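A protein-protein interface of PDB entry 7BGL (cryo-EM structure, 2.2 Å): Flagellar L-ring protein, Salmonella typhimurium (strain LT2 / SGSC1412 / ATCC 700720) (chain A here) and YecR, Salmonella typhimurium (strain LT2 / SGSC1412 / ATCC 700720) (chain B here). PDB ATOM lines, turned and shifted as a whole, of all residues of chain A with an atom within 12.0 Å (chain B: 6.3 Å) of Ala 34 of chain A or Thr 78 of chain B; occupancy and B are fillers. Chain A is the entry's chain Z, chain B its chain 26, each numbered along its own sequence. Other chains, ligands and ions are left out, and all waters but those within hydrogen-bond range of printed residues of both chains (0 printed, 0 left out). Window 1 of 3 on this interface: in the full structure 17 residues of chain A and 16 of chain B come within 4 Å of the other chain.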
ATOM      1  N   ALA A  27      -1.869 -25.630   1.678  1.00  0.00           N
ATOM      2  CA  ALA A  27      -2.876 -26.313   2.474  1.00  0.00           C
ATOM      3  C   ALA A  27      -4.042 -26.703   1.579  1.00  0.00           C
ATOM      4  O   ALA A  27      -4.303 -26.061   0.557  1.00  0.00           O
ATOM      5  CB  ALA A  27      -3.366 -25.440   3.634  1.00  0.00           C
ATOM      6  N   LYS A  28      -4.741 -27.764   1.977  1.00  0.00           N
ATOM      7  CA  LYS A  28      -5.901 -28.253   1.247  1.00  0.00           C
ATOM      8  C   LYS A  28      -7.161 -27.949   2.038  1.00  0.00           C
ATOM      9  O   LYS A  28      -7.308 -28.444   3.166  1.00  0.00           O
ATOM     10  CB  LYS A  28      -5.784 -29.753   0.987  1.00  0.00           C
ATOM     11  CG  LYS A  28      -4.417 -30.197   0.499  1.00  0.00           C
ATOM     12  CD  LYS A  28      -4.407 -31.680   0.172  1.00  0.00           C
ATOM     13  CE  LYS A  28      -5.010 -31.951  -1.196  1.00  0.00           C
ATOM     14  NZ  LYS A  28      -4.205 -31.342  -2.289  1.00  0.00           N
ATOM     15  N   PRO A  29      -8.086 -27.152   1.507  1.00  0.00           N
ATOM     16  CA  PRO A  29      -9.331 -26.888   2.237  1.00  0.00           C
ATOM     17  C   PRO A  29     -10.122 -28.170   2.447  1.00  0.00           C
ATOM     18  O   PRO A  29     -10.095 -29.085   1.622  1.00  0.00           O
ATOM     19  CB  PRO A  29     -10.077 -25.909   1.324  1.00  0.00           C
ATOM     20  CG  PRO A  29      -9.512 -26.155  -0.036  1.00  0.00           C
ATOM     21  CD  PRO A  29      -8.073 -26.517   0.180  1.00  0.00           C
ATOM     22  N   LEU A  30     -10.832 -28.230   3.577  1.00  0.00           N
ATOM     23  CA  LEU A  30     -11.608 -29.428   3.884  1.00  0.00           C
ATOM     24  C   LEU A  30     -12.677 -29.685   2.831  1.00  0.00           C
ATOM     25  O   LEU A  30     -13.010 -30.844   2.558  1.00  0.00           O
ATOM     26  CB  LEU A  30     -12.242 -29.316   5.271  1.00  0.00           C
ATOM     27  CG  LEU A  30     -13.108 -28.095   5.576  1.00  0.00           C
ATOM     28  CD1 LEU A  30     -14.019 -28.377   6.755  1.00  0.00           C
ATOM     29  CD2 LEU A  30     -12.231 -26.896   5.867  1.00  0.00           C
ATOM     30  N   VAL A  31     -13.221 -28.633   2.229  1.00  0.00           N
ATOM     31  CA  VAL A  31     -14.209 -28.790   1.149  1.00  0.00           C
ATOM     32  C   VAL A  31     -13.405 -28.893  -0.140  1.00  0.00           C
ATOM     33  O   VAL A  31     -13.187 -27.922  -0.869  1.00  0.00           O
ATOM     34  CB  VAL A  31     -15.230 -27.648   1.126  1.00  0.00           C
ATOM     35  CG1 VAL A  31     -16.199 -27.832  -0.030  1.00  0.00           C
ATOM     36  CG2 VAL A  31     -15.977 -27.579   2.447  1.00  0.00           C
ATOM     37  N   GLN A  32     -12.950 -30.106  -0.429  1.00  0.00           N
ATOM     38  CA  GLN A  32     -12.137 -30.366  -1.606  1.00  0.00           C
ATOM     39  C   GLN A  32     -13.017 -30.615  -2.826  1.00  0.00           C
ATOM     40  O   GLN A  32     -14.214 -30.886  -2.717  1.00  0.00           O
ATOM     41  CB  GLN A  32     -11.215 -31.562  -1.373  1.00  0.00           C
ATOM     42  CG  GLN A  32     -10.267 -31.393  -0.199  1.00  0.00           C
ATOM     43  CD  GLN A  32      -9.329 -32.571  -0.035  1.00  0.00           C
ATOM     44  OE1 GLN A  32      -9.279 -33.462  -0.884  1.00  0.00           O
ATOM     45  NE2 GLN A  32      -8.578 -32.583   1.059  1.00  0.00           N
ATOM     46  N   GLY A  33     -12.399 -30.519  -3.998  1.00  0.00           N
ATOM     47  CA  GLY A  33     -13.108 -30.722  -5.243  1.00  0.00           C
ATOM     48  C   GLY A  33     -13.780 -29.460  -5.739  1.00  0.00           C
ATOM     49  O   GLY A  33     -13.794 -28.411  -5.089  1.00  0.00           O
ATOM     50  N   ALA A  34     -14.355 -29.572  -6.932  1.00  0.00           N
ATOM     51  CA  ALA A  34     -15.041 -28.441  -7.535  1.00  0.00           C
ATOM     52  C   ALA A  34     -16.261 -28.054  -6.710  1.00  0.00           C
ATOM     53  O   ALA A  34     -16.982 -28.910  -6.193  1.00  0.00           O
ATOM     54  CB  ALA A  34     -15.459 -28.773  -8.966  1.00  0.00           C
ATOM     55  N   THR A  35     -16.489 -26.748  -6.589  1.00  0.00           N
ATOM     56  CA  THR A  35     -17.662 -26.216  -5.911  1.00  0.00           C
ATOM     57  C   THR A  35     -18.786 -25.887  -6.881  1.00  0.00           C
ATOM     58  O   THR A  35     -19.737 -25.197  -6.503  1.00  0.00           O
ATOM     59  CB  THR A  35     -17.293 -24.970  -5.104  1.00  0.00           C
ATOM     60  OG1 THR A  35     -16.858 -23.933  -5.993  1.00  0.00           O
ATOM     61  CG2 THR A  35     -16.184 -25.284  -4.112  1.00  0.00           C
ATOM     62  N   THR A  36     -18.690 -26.353  -8.124  1.00  0.00           N
ATOM     63  CA  THR A  36     -19.661 -26.046  -9.162  1.00  0.00           C
ATOM     64  C   THR A  36     -20.045 -27.310  -9.911  1.00  0.00           C
ATOM     65  O   THR A  36     -19.231 -28.226 -10.065  1.00  0.00           O
ATOM     66  CB  THR A  36     -19.104 -25.023 -10.151  1.00  0.00           C
ATOM     67  OG1 THR A  36     -17.674 -25.025 -10.085  1.00  0.00           O
ATOM     68  CG2 THR A  36     -19.609 -23.649  -9.811  1.00  0.00           C
ATOM     69  N   ALA A  37     -21.289 -27.352 -10.376  1.00  0.00           N
ATOM     70  CA  ALA A  37     -21.785 -28.433 -11.215  1.00  0.00           C
ATOM     71  C   ALA A  37     -22.471 -27.823 -12.426  1.00  0.00           C
ATOM     72  O   ALA A  37     -23.378 -26.997 -12.279  1.00  0.00           O
ATOM     73  CB  ALA A  37     -22.747 -29.336 -10.441  1.00  0.00           C
ATOM     74  N   GLN A  38     -22.033 -28.215 -13.613  1.00  0.00           N
ATOM     75  CA  GLN A  38     -22.679 -27.747 -14.830  1.00  0.00           C
ATOM     76  C   GLN A  38     -23.955 -28.545 -15.071  1.00  0.00           C
ATOM     77  O   GLN A  38     -23.904 -29.778 -15.147  1.00  0.00           O
ATOM     78  CB  GLN A  38     -21.737 -27.882 -16.024  1.00  0.00           C
ATOM     79  CG  GLN A  38     -20.656 -26.817 -16.090  1.00  0.00           C
ATOM     80  CD  GLN A  38     -21.143 -25.462 -15.617  1.00  0.00           C
ATOM     81  OE1 GLN A  38     -22.024 -24.858 -16.228  1.00  0.00           O
ATOM     82  NE2 GLN A  38     -20.568 -24.975 -14.524  1.00  0.00           N
ATOM     83  N   PRO A  39     -25.109 -27.893 -15.189  1.00  0.00           N
ATOM     84  CA  PRO A  39     -26.352 -28.638 -15.419  1.00  0.00           C
ATOM     85  C   PRO A  39     -26.316 -29.398 -16.736  1.00  0.00           C
ATOM     86  O   PRO A  39     -25.727 -28.953 -17.724  1.00  0.00           O
ATOM     87  CB  PRO A  39     -27.426 -27.544 -15.429  1.00  0.00           C
ATOM     88  CG  PRO A  39     -26.690 -26.290 -15.762  1.00  0.00           C
ATOM     89  CD  PRO A  39     -25.334 -26.439 -15.144  1.00  0.00           C
ATOM     90  N   VAL B  76     -14.714 -26.467 -15.640  1.00  0.00           N
ATOM     91  CA  VAL B  76     -14.838 -25.836 -14.333  1.00  0.00           C
ATOM     92  C   VAL B  76     -13.486 -25.906 -13.638  1.00  0.00           C
ATOM     93  O   VAL B  76     -12.899 -26.987 -13.520  1.00  0.00           O
ATOM     94  CB  VAL B  76     -15.926 -26.508 -13.477  1.00  0.00           C
ATOM     95  CG1 VAL B  76     -15.915 -25.937 -12.072  1.00  0.00           C
ATOM     96  CG2 VAL B  76     -17.293 -26.328 -14.120  1.00  0.00           C
ATOM     97  N   GLY B  77     -12.997 -24.756 -13.179  1.00  0.00           N
ATOM     98  CA  GLY B  77     -11.710 -24.699 -12.516  1.00  0.00           C
ATOM     99  C   GLY B  77     -11.791 -24.239 -11.075  1.00  0.00           C
ATOM    100  O   GLY B  77     -12.171 -23.098 -10.800  1.00  0.00           O
ATOM    101  N   THR B  78     -11.435 -25.123 -10.145  1.00  0.00           N
ATOM    102  CA  THR B  78     -11.420 -24.813  -8.723  1.00  0.00           C
ATOM    103  C   THR B  78     -10.026 -25.073  -8.171  1.00  0.00           C
ATOM    104  O   THR B  78      -9.437 -26.127  -8.436  1.00  0.00           O
ATOM    105  CB  THR B  78     -12.453 -25.647  -7.959  1.00  0.00           C
ATOM    106  OG1 THR B  78     -12.107 -27.035  -8.043  1.00  0.00           O
ATOM    107  CG2 THR B  78     -13.843 -25.438  -8.543  1.00  0.00           C
ATOM    108  N   CYS B  79      -9.505 -24.117  -7.408  1.00  0.00           N
ATOM    109  CA  CYS B  79      -8.175 -24.268  -6.833  1.00  0.00           C
ATOM    110  C   CYS B  79      -8.142 -25.439  -5.860  1.00  0.00           C
ATOM    111  O   CYS B  79      -9.056 -25.626  -5.052  1.00  0.00           O
ATOM    112  CB  CYS B  79      -7.757 -22.980  -6.124  1.00  0.00           C
ATOM    113  SG  CYS B  79      -5.973 -22.805  -5.887  1.00  0.00           S
ATOM    114  N   SER B  80      -7.074 -26.234  -5.943  1.00  0.00           N
ATOM    115  CA  SER B  80      -6.898 -27.388  -5.073  1.00  0.00           C
ATOM    116  C   SER B  80      -5.773 -27.227  -4.062  1.00  0.00           C
ATOM    117  O   SER B  80      -5.773 -27.930  -3.047  1.00  0.00           O
ATOM    118  CB  SER B  80      -6.638 -28.651  -5.906  1.00  0.00           C
ATOM    119  OG  SER B  80      -5.487 -28.501  -6.717  1.00  0.00           O
ATOM    120  N   ILE B  81      -4.820 -26.331  -4.311  1.00  0.00           N
ATOM    121  CA  ILE B  81      -3.718 -26.066  -3.396  1.00  0.00           C
ATOM    122  C   ILE B  81      -3.682 -24.571  -3.114  1.00  0.00           C
ATOM    123  O   ILE B  81      -3.711 -23.760  -4.046  1.00  0.00           O
ATOM    124  CB  ILE B  81      -2.368 -26.540  -3.967  1.00  0.00           C
ATOM    125  CG1 ILE B  81      -2.427 -28.029  -4.310  1.00  0.00           C
ATOM    126  CG2 ILE B  81      -1.247 -26.264  -2.979  1.00  0.00           C
ATOM    127  CD1 ILE B  81      -2.490 -28.929  -3.099  1.00  0.00           C
ATOM    128  N   CYS B  87      -2.642 -19.434  -5.760  1.00  0.00           N
ATOM    129  CA  CYS B  87      -3.275 -20.693  -6.166  1.00  0.00           C
ATOM    130  C   CYS B  87      -2.203 -21.529  -6.862  1.00  0.00           C
ATOM    131  O   CYS B  87      -1.970 -21.384  -8.065  1.00  0.00           O
ATOM    132  CB  CYS B  87      -4.479 -20.446  -7.065  1.00  0.00           C
ATOM    133  SG  CYS B  87      -5.325 -21.947  -7.610  1.00  0.00           S
ATOM    134  N   ASN B  89      -2.103 -24.773  -7.555  1.00  0.00           N
ATOM    135  CA  ASN B  89      -2.664 -25.694  -8.530  1.00  0.00           C
ATOM    136  C   ASN B  89      -4.148 -25.416  -8.712  1.00  0.00           C
ATOM    137  O   ASN B  89      -4.841 -25.017  -7.773  1.00  0.00           O
ATOM    138  CB  ASN B  89      -2.457 -27.155  -8.107  1.00  0.00           C
ATOM    139  CG  ASN B  89      -2.971 -28.139  -9.138  1.00  0.00           C
ATOM    140  OD1 ASN B  89      -2.569 -28.104 -10.302  1.00  0.00           O
ATOM    141  ND2 ASN B  89      -3.869 -29.021  -8.718  1.00  0.00           N
ATOM    142  N   THR B  90      -4.630 -25.634  -9.934  1.00  0.00           N
ATOM    143  CA  THR B  90      -6.037 -25.463 -10.264  1.00  0.00           C
ATOM    144  C   THR B  90      -6.554 -26.738 -10.911  1.00  0.00           C
ATOM    145  O   THR B  90      -5.925 -27.271 -11.830  1.00  0.00           O
ATOM    146  CB  THR B  90      -6.250 -24.271 -11.204  1.00  0.00           C
ATOM    147  OG1 THR B  90      -5.787 -23.073 -10.571  1.00  0.00           O
ATOM    148  CG2 THR B  90      -7.724 -24.121 -11.545  1.00  0.00           C
ATOM    149  N   ARG B  91      -7.696 -27.223 -10.434  1.00  0.00           N
ATOM    150  CA  ARG B  91      -8.322 -28.414 -10.992  1.00  0.00           C
ATOM    151  C   ARG B  91      -9.418 -28.008 -11.968  1.00  0.00           C
ATOM    152  O   ARG B  91     -10.311 -27.229 -11.619  1.00  0.00           O
ATOM    153  CB  ARG B  91      -8.901 -29.293  -9.885  1.00  0.00           C
ATOM    154  CG  ARG B  91      -7.856 -29.954  -9.004  1.00  0.00           C
ATOM    155  CD  ARG B  91      -7.278 -31.188  -9.672  1.00  0.00           C
ATOM    156  NE  ARG B  91      -6.281 -31.844  -8.835  1.00  0.00           N
ATOM    157  CZ  ARG B  91      -6.569 -32.638  -7.813  1.00  0.00           C
ATOM    158  NH1 ARG B  91      -7.820 -32.897  -7.470  1.00  0.00           N
ATOM    159  NH2 ARG B  91      -5.577 -33.185  -7.116  1.00  0.00           N
ATOM    160  N   PHE B  92      -9.349 -28.536 -13.187  1.00  0.00           N
ATOM    161  CA  PHE B  92     -10.345 -28.277 -14.215  1.00  0.00           C
ATOM    162  C   PHE B  92     -11.106 -29.564 -14.495  1.00  0.00           C
ATOM    163  O   PHE B  92     -10.496 -30.617 -14.715  1.00  0.00           O
ATOM    164  CB  PHE B  92      -9.696 -27.746 -15.494  1.00  0.00           C
ATOM    165  CG  PHE B  92      -9.199 -26.334 -15.378  1.00  0.00           C
ATOM    166  CD1 PHE B  92      -7.909 -26.074 -14.949  1.00  0.00           C
ATOM    167  CD2 PHE B  92     -10.022 -25.269 -15.694  1.00  0.00           C
ATOM    168  CE1 PHE B  92      -7.449 -24.777 -14.841  1.00  0.00           C
ATOM    169  CE2 PHE B  92      -9.568 -23.969 -15.587  1.00  0.00           C
ATOM    170  CZ  PHE B  92      -8.280 -23.722 -15.160  1.00  0.00           C
ATOM    171  N   THR B  93     -12.433 -29.473 -14.487  1.00  0.00           N
ATOM    172  CA  THR B  93     -13.307 -30.627 -14.618  1.00  0.00           C
ATOM    173  C   THR B  93     -14.084 -30.571 -15.928  1.00  0.00           C
ATOM    174  O   THR B  93     -14.500 -29.502 -16.383  1.00  0.00           O
ATOM    175  CB  THR B  93     -14.289 -30.712 -13.446  1.00  0.00           C
ATOM    176  OG1 THR B  93     -15.249 -29.652 -13.546  1.00  0.00           O
ATOM    177  CG2 THR B  93     -13.551 -30.594 -12.122  1.00  0.00           C
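Printed residues of chain A that touch a printed residue of chain B: Ala 27, Lys 28, Gly 33, Ala 34, Thr 35, Thr 36 and Gln 38.
Hydrophobic or aromatic side chains of chain A that line the printed part of chain B: Ala 34.
Among the printed residues, 8 pairs touch across the chains.
Of the printed residues of chain B, Ala 27 of chain A touches Ile 81.
Leu 30 of chain A touches none of the printed residues of chain B.
Of the printed residues of chain B, Gly 33 of chain A touches Thr 78.
Of chain B, only Thr 78 (3.3 Å) comes within 4 Å of Ala 34 of chain A.
Printed residues of chain B within 4 Å of Thr 35 of chain A: Thr 78.
Of the printed residues of chain B, Gln 38 of chain A touches Val 76 (3.6 Å).
Of chain A, only Thr 36 (2.8 Å) and Gln 38 (3.6 Å) come within 4 Å of Val 76 of chain B.
No residue of chain A comes within 4 Å of Gly 77 of chain B.
Thr 78 of chain B touches three residues of chain A.
No residue of chain A comes within 4 Å of Cys 79 of chain B.
Ser 80 of chain B touches one residue of chain A.
Of the printed residues of chain A, Ile 81 of chain B touches Ala 27 and Lys 28.
Thr 90 of chain B touches none of the printed residues of chain A.
No residue of chain A comes within 4 Å of Phe 92 of chain B.
The nearest residue of chain B that does not touch Ala 34 of chain A is Thr 93 of chain B (4.1 Å).
The nearest residue of chain A that does not touch Thr 78 of chain B is Thr 36 of chain A (4.2 Å).
The nearest printed residue of chain B that does not touch Ala 27 of chain A is Ser 80 of chain B (4.3 Å).
The side-chain sulfur of Cys 87 of chain B is disulfide-bonded to the side-chain sulfur of Cys 79 of chain B (2.0 Å).
The backbone NH (N) of Thr 78 of chain B sits at hydrogen-bond distance from the backbone carbonyl oxygen (O) of Arg 91 of chain B, at 2.8 Å.
OG of Ser 80 of chain B lies within hydrogen-bond range of ND2 of Asn 89 of chain B, 2.6 Å away.
The backbone carbonyl oxygen (O) of Val 76 of chain B is in hydrogen-bond range of the backbone NH (N) of Thr 93 of chain B, 2.7 Å away.
O of Ala 27 of chain A touches CA of Ile 81 of chain B, at 3.996 Å.
O of Ser 80 of chain B touches NZ of Lys 28 of chain A, at 3.8 Å.
NZ of Lys 28 of chain A touches CD1 of Ile 81 of chain B, at 3.1 Å.
Thr 78 of chain B touches Gly 33 of chain A.
Ala 34 of chain A touches Thr 78 of chain B (CA to OG1, 3.3 Å).
Thr 78 of chain B touches Thr 35 of chain A.
Thr 36 of chain A touches Val 76 of chain B (OG1 to CG1, 2.8 Å).
Gln 38 of chain A touches Val 76 of chain B.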
